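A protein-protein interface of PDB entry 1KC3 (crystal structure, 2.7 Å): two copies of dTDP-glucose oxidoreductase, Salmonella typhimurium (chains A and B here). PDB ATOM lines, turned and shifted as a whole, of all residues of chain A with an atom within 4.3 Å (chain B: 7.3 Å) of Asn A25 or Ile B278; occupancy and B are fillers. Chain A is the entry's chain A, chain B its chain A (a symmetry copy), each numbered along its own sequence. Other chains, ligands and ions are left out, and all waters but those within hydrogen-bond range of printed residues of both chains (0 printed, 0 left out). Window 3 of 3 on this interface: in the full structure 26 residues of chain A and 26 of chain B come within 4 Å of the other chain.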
ATOM      1  N   MET A   1       5.008  23.899 -13.266  1.00  0.00           N
ATOM      2  CA  MET A   1       5.159  25.338 -13.527  1.00  0.00           C
ATOM      3  C   MET A   1       4.458  25.749 -14.818  1.00  0.00           C
ATOM      4  O   MET A   1       4.362  25.009 -15.772  1.00  0.00           O
ATOM      5  CB  MET A   1       6.634  25.721 -13.531  1.00  0.00           C
ATOM      6  CG  MET A   1       7.379  25.263 -14.735  1.00  0.00           C
ATOM      7  SD  MET A   1       7.593  26.652 -15.836  1.00  0.00           S
ATOM      8  CE  MET A   1       9.220  26.152 -16.657  1.00  0.00           C
ATOM      9  N   ASN A   2       3.959  26.970 -14.764  1.00  0.00           N
ATOM     10  CA  ASN A   2       3.097  27.538 -15.799  1.00  0.00           C
ATOM     11  C   ASN A   2       3.792  28.330 -16.878  1.00  0.00           C
ATOM     12  O   ASN A   2       4.477  29.347 -16.614  1.00  0.00           O
ATOM     13  CB  ASN A   2       1.993  28.369 -15.165  1.00  0.00           C
ATOM     14  CG  ASN A   2       1.042  27.509 -14.384  1.00  0.00           C
ATOM     15  OD1 ASN A   2       0.308  26.702 -14.957  1.00  0.00           O
ATOM     16  ND2 ASN A   2       1.089  27.629 -13.069  1.00  0.00           N
ATOM     17  N   ILE A   3       3.518  27.907 -18.084  1.00  0.00           N
ATOM     18  CA  ILE A   3       4.026  28.537 -19.252  1.00  0.00           C
ATOM     19  C   ILE A   3       2.895  29.224 -19.926  1.00  0.00           C
ATOM     20  O   ILE A   3       1.833  28.652 -20.049  1.00  0.00           O
ATOM     21  CB  ILE A   3       4.613  27.492 -20.275  1.00  0.00           C
ATOM     22  CG1 ILE A   3       5.609  26.613 -19.554  1.00  0.00           C
ATOM     23  CG2 ILE A   3       5.279  28.239 -21.420  1.00  0.00           C
ATOM     24  CD1 ILE A   3       6.446  25.643 -20.427  1.00  0.00           C
ATOM     25  N   ALA A  21       5.026  21.875 -24.391  1.00  0.00           N
ATOM     26  CA  ALA A  21       4.058  20.916 -23.776  1.00  0.00           C
ATOM     27  C   ALA A  21       4.576  20.075 -22.584  1.00  0.00           C
ATOM     28  O   ALA A  21       3.807  19.863 -21.693  1.00  0.00           O
ATOM     29  CB  ALA A  21       3.416  19.964 -24.888  1.00  0.00           C
ATOM     30  N   PRO A  22       5.792  19.511 -22.639  1.00  0.00           N
ATOM     31  CA  PRO A  22       6.367  18.800 -21.489  1.00  0.00           C
ATOM     32  C   PRO A  22       7.201  19.689 -20.526  1.00  0.00           C
ATOM     33  O   PRO A  22       7.458  19.305 -19.350  1.00  0.00           O
ATOM     34  CB  PRO A  22       7.295  17.760 -22.144  1.00  0.00           C
ATOM     35  CG  PRO A  22       7.584  18.257 -23.612  1.00  0.00           C
ATOM     36  CD  PRO A  22       6.694  19.431 -23.818  1.00  0.00           C
ATOM     37  N   GLY A  24       6.470  22.533 -19.172  1.00  0.00           N
ATOM     38  CA  GLY A  24       5.564  22.931 -18.067  1.00  0.00           C
ATOM     39  C   GLY A  24       4.118  23.029 -18.548  1.00  0.00           C
ATOM     40  O   GLY A  24       3.834  22.927 -19.782  1.00  0.00           O
ATOM     41  N   ASN A  25       3.216  23.258 -17.568  1.00  0.00           N
ATOM     42  CA  ASN A  25       1.758  23.417 -17.797  1.00  0.00           C
ATOM     43  C   ASN A  25       1.504  24.602 -18.807  1.00  0.00           C
ATOM     44  O   ASN A  25       1.957  25.768 -18.599  1.00  0.00           O
ATOM     45  CB  ASN A  25       0.987  23.532 -16.511  1.00  0.00           C
ATOM     46  CG  ASN A  25       0.576  22.157 -15.973  1.00  0.00           C
ATOM     47  OD1 ASN A  25      -0.133  21.369 -16.659  1.00  0.00           O
ATOM     48  ND2 ASN A  25       1.024  21.842 -14.744  1.00  0.00           N
ATOM     49  N   LEU A  26       0.872  24.251 -19.945  1.00  0.00           N
ATOM     50  CA  LEU A  26       0.791  25.144 -21.132  1.00  0.00           C
ATOM     51  C   LEU A  26      -0.625  25.723 -21.438  1.00  0.00           C
ATOM     52  O   LEU A  26      -1.606  24.968 -21.634  1.00  0.00           O
ATOM     53  CB  LEU A  26       1.370  24.486 -22.386  1.00  0.00           C
ATOM     54  CG  LEU A  26       1.353  25.386 -23.650  1.00  0.00           C
ATOM     55  CD1 LEU A  26       2.027  26.753 -23.517  1.00  0.00           C
ATOM     56  CD2 LEU A  26       2.020  24.739 -24.829  1.00  0.00           C
ATOM     57  N   ILE A  27      -0.682  27.053 -21.397  1.00  0.00           N
ATOM     58  CA  ILE A  27      -1.822  27.804 -21.839  1.00  0.00           C
ATOM     59  C   ILE A  27      -1.291  28.437 -23.100  1.00  0.00           C
ATOM     60  O   ILE A  27      -0.275  29.157 -23.074  1.00  0.00           O
ATOM     61  CB  ILE A  27      -2.275  28.815 -20.786  1.00  0.00           C
ATOM     62  CG1 ILE A  27      -2.971  28.049 -19.665  1.00  0.00           C
ATOM     63  CG2 ILE A  27      -3.215  29.850 -21.358  1.00  0.00           C
ATOM     64  CD1 ILE A  27      -2.480  28.427 -18.330  1.00  0.00           C
ATOM     65  N   LEU B 191       5.955  13.822 -28.468  1.00  0.00           N
ATOM     66  CA  LEU B 191       6.158  13.774 -26.997  1.00  0.00           C
ATOM     67  C   LEU B 191       7.351  12.864 -26.669  1.00  0.00           C
ATOM     68  O   LEU B 191       8.274  13.290 -26.005  1.00  0.00           O
ATOM     69  CB  LEU B 191       4.906  13.380 -26.211  1.00  0.00           C
ATOM     70  CG  LEU B 191       5.190  13.237 -24.678  1.00  0.00           C
ATOM     71  CD1 LEU B 191       5.326  14.597 -24.067  1.00  0.00           C
ATOM     72  CD2 LEU B 191       4.240  12.414 -23.941  1.00  0.00           C
ATOM     73  N   CYS B 195      10.667  14.732 -24.852  1.00  0.00           N
ATOM     74  CA  CYS B 195      11.066  14.174 -23.562  1.00  0.00           C
ATOM     75  C   CYS B 195      12.386  13.432 -23.586  1.00  0.00           C
ATOM     76  O   CYS B 195      13.124  13.519 -22.615  1.00  0.00           O
ATOM     77  CB  CYS B 195       9.997  13.159 -23.083  1.00  0.00           C
ATOM     78  SG  CYS B 195       8.533  14.057 -22.496  1.00  0.00           S
ATOM     79  N   LEU B 215       6.970   5.938 -19.937  1.00  0.00           N
ATOM     80  CA  LEU B 215       6.769   7.218 -20.618  1.00  0.00           C
ATOM     81  C   LEU B 215       5.632   7.157 -21.660  1.00  0.00           C
ATOM     82  O   LEU B 215       5.825   6.646 -22.775  1.00  0.00           O
ATOM     83  CB  LEU B 215       8.083   7.709 -21.245  1.00  0.00           C
ATOM     84  CG  LEU B 215       8.057   9.003 -22.051  1.00  0.00           C
ATOM     85  CD1 LEU B 215       7.467  10.182 -21.280  1.00  0.00           C
ATOM     86  CD2 LEU B 215       9.504   9.241 -22.444  1.00  0.00           C
ATOM     87  N   PHE B 271       8.666   9.213 -14.054  1.00  0.00           N
ATOM     88  CA  PHE B 271       9.298  10.056 -15.112  1.00  0.00           C
ATOM     89  C   PHE B 271       9.172  11.534 -14.778  1.00  0.00           C
ATOM     90  O   PHE B 271      10.093  12.298 -14.946  1.00  0.00           O
ATOM     91  CB  PHE B 271       8.681   9.857 -16.510  1.00  0.00           C
ATOM     92  CG  PHE B 271       9.430  10.603 -17.634  1.00  0.00           C
ATOM     93  CD1 PHE B 271      10.521   9.985 -18.323  1.00  0.00           C
ATOM     94  CD2 PHE B 271       9.067  11.927 -17.999  1.00  0.00           C
ATOM     95  CE1 PHE B 271      11.214  10.615 -19.302  1.00  0.00           C
ATOM     96  CE2 PHE B 271       9.775  12.557 -19.016  1.00  0.00           C
ATOM     97  CZ  PHE B 271      10.879  11.881 -19.642  1.00  0.00           C
ATOM     98  N   GLN B 272       7.993  11.899 -14.332  1.00  0.00           N
ATOM     99  CA  GLN B 272       7.644  13.277 -14.076  1.00  0.00           C
ATOM    100  C   GLN B 272       8.549  13.869 -12.998  1.00  0.00           C
ATOM    101  O   GLN B 272       9.210  14.895 -13.233  1.00  0.00           O
ATOM    102  CB  GLN B 272       6.192  13.374 -13.726  1.00  0.00           C
ATOM    103  CG  GLN B 272       5.293  13.057 -14.896  1.00  0.00           C
ATOM    104  CD  GLN B 272       3.822  13.141 -14.496  1.00  0.00           C
ATOM    105  OE1 GLN B 272       3.365  14.183 -13.990  1.00  0.00           O
ATOM    106  NE2 GLN B 272       3.090  12.050 -14.680  1.00  0.00           N
ATOM    107  N   PHE B 275      12.676  13.581 -14.183  1.00  0.00           N
ATOM    108  CA  PHE B 275      13.091  14.532 -15.234  1.00  0.00           C
ATOM    109  C   PHE B 275      12.522  15.995 -15.144  1.00  0.00           C
ATOM    110  O   PHE B 275      12.941  16.897 -15.867  1.00  0.00           O
ATOM    111  CB  PHE B 275      12.876  13.871 -16.603  1.00  0.00           C
ATOM    112  CG  PHE B 275      13.776  12.684 -16.811  1.00  0.00           C
ATOM    113  CD1 PHE B 275      13.335  11.418 -16.562  1.00  0.00           C
ATOM    114  CD2 PHE B 275      15.102  12.861 -17.131  1.00  0.00           C
ATOM    115  CE1 PHE B 275      14.224  10.334 -16.660  1.00  0.00           C
ATOM    116  CE2 PHE B 275      15.966  11.788 -17.273  1.00  0.00           C
ATOM    117  CZ  PHE B 275      15.534  10.529 -17.022  1.00  0.00           C
ATOM    118  N   ASP B 276      11.657  16.212 -14.167  1.00  0.00           N
ATOM    119  CA  ASP B 276      10.999  17.527 -13.902  1.00  0.00           C
ATOM    120  C   ASP B 276      10.155  17.917 -15.111  1.00  0.00           C
ATOM    121  O   ASP B 276      10.138  19.068 -15.534  1.00  0.00           O
ATOM    122  CB  ASP B 276      12.061  18.595 -13.601  1.00  0.00           C
ATOM    123  CG  ASP B 276      11.540  19.758 -12.810  1.00  0.00           C
ATOM    124  OD1 ASP B 276      12.316  20.281 -11.947  1.00  0.00           O
ATOM    125  OD2 ASP B 276      10.397  20.233 -12.974  1.00  0.00           O
ATOM    126  N   LEU B 277       9.513  16.923 -15.692  1.00  0.00           N
ATOM    127  CA  LEU B 277       8.834  17.073 -16.961  1.00  0.00           C
ATOM    128  C   LEU B 277       7.354  16.843 -16.817  1.00  0.00           C
ATOM    129  O   LEU B 277       6.904  16.061 -15.992  1.00  0.00           O
ATOM    130  CB  LEU B 277       9.411  16.110 -18.034  1.00  0.00           C
ATOM    131  CG  LEU B 277      10.734  16.492 -18.682  1.00  0.00           C
ATOM    132  CD1 LEU B 277      11.426  15.376 -19.663  1.00  0.00           C
ATOM    133  CD2 LEU B 277      10.611  17.866 -19.434  1.00  0.00           C
ATOM    134  N   ILE B 278       6.639  17.499 -17.712  1.00  0.00           N
ATOM    135  CA  ILE B 278       5.186  17.366 -17.876  1.00  0.00           C
ATOM    136  C   ILE B 278       4.837  16.385 -19.002  1.00  0.00           C
ATOM    137  O   ILE B 278       5.580  16.210 -20.014  1.00  0.00           O
ATOM    138  CB  ILE B 278       4.462  18.781 -18.056  1.00  0.00           C
ATOM    139  CG1 ILE B 278       4.737  19.666 -16.849  1.00  0.00           C
ATOM    140  CG2 ILE B 278       2.949  18.695 -18.212  1.00  0.00           C
ATOM    141  CD1 ILE B 278       4.537  18.935 -15.480  1.00  0.00           C
ATOM    142  N   LEU B 279       3.715  15.706 -18.793  1.00  0.00           N
ATOM    143  CA  LEU B 279       3.197  14.612 -19.673  1.00  0.00           C
ATOM    144  C   LEU B 279       1.665  14.898 -19.847  1.00  0.00           C
ATOM    145  O   LEU B 279       0.801  14.378 -19.088  1.00  0.00           O
ATOM    146  CB  LEU B 279       3.515  13.222 -19.115  1.00  0.00           C
ATOM    147  CG  LEU B 279       5.000  12.912 -19.029  1.00  0.00           C
ATOM    148  CD1 LEU B 279       5.227  11.566 -18.325  1.00  0.00           C
ATOM    149  CD2 LEU B 279       5.638  12.892 -20.399  1.00  0.00           C
ATOM    150  N   PRO B 280       1.339  15.731 -20.855  1.00  0.00           N
ATOM    151  CA  PRO B 280      -0.042  16.184 -21.011  1.00  0.00           C
ATOM    152  C   PRO B 280      -1.031  15.186 -21.579  1.00  0.00           C
ATOM    153  O   PRO B 280      -0.642  14.200 -22.214  1.00  0.00           O
ATOM    154  CB  PRO B 280       0.109  17.352 -21.932  1.00  0.00           C
ATOM    155  CG  PRO B 280       1.604  17.604 -21.933  1.00  0.00           C
ATOM    156  CD  PRO B 280       2.186  16.288 -21.925  1.00  0.00           C
ATOM    157  N   GLN B 281      -2.294  15.516 -21.380  1.00  0.00           N
ATOM    158  CA  GLN B 281      -3.401  14.675 -21.730  1.00  0.00           C
ATOM    159  C   GLN B 281      -3.350  14.280 -23.195  1.00  0.00           C
ATOM    160  O   GLN B 281      -3.038  15.127 -24.073  1.00  0.00           O
ATOM    161  CB  GLN B 281      -4.709  15.360 -21.387  1.00  0.00           C
ATOM    162  CG  GLN B 281      -4.935  15.415 -19.902  1.00  0.00           C
ATOM    163  CD  GLN B 281      -5.008  14.026 -19.213  1.00  0.00           C
ATOM    164  OE1 GLN B 281      -5.865  13.200 -19.543  1.00  0.00           O
ATOM    165  NE2 GLN B 281      -4.104  13.781 -18.255  1.00  0.00           N
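O of Ala A21 touches CG2 of Ile B278, at 3.8 Å. CG of Pro B280 touches O of Ala A21 (3.2 Å). Pro A22 touches Cys B195 (CB to SG, 3.9 Å). Pro A22 touches Leu B277. Gly A24 touches Ile B278. Ile B278 touches Asn A25.
Of the 12 printed residues of chain B, 4 touch a printed residue of chain A. Among the printed residues, 7 pairs touch across the chains. Among the printed residues, no Asp or Glu carboxylate lies within 4 Å of a Lys or Arg side-chain nitrogen of the other chain.
No position is printed for both chains. Of the 7 pairs that touch across the chains among the printed residues, none has its exchanged pair printed and touching as well.
O of Met A1 is in hydrogen-bond range of N of Asn A25 (2.8 Å). The backbone NH (N) of Ile A3 lies within hydrogen-bond range of the backbone carbonyl oxygen (O) of Asn A25, 2.7 Å away. The side-chain sulfur (SG) of Cys B195 lies close to the backbone carbonyl oxygen (O) of Leu B191 (3.6 Å). The backbone carbonyl oxygen (O) of Gln B272 is in hydrogen-bond range of the backbone NH (N) of Leu B277, at 3.2 Å.
Asn A25 touches just one residue of chain B: Ile B278. Of chain A, only Ala A21, Pro A22, Gly A24 and Asn A25 come within 4 Å of Ile B278. Printed residues of chain B within 4 Å of Gly A24: Ile B278 (3.6 Å). Of the printed residues of chain B, Pro A22 touches Cys B195, Leu B277 and Ile B278. Printed residues of chain A within 4 Å of Leu B277: Pro A22 (3.5 Å). Printed residues of chain A within 4 Å of Cys B195: Pro A22. Asp B276 touches none of the printed residues of chain A. Phe B275 touches none of the printed residues of chain A. The nearest residue of chain B that does not touch Asn A25 is Pro B280 (6.6 Å).
The backbone carbonyl oxygen (O) of Pro A22 sits at hydrogen-bond distance from the backbone NH (N) of Ile B278 (2.6 Å).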
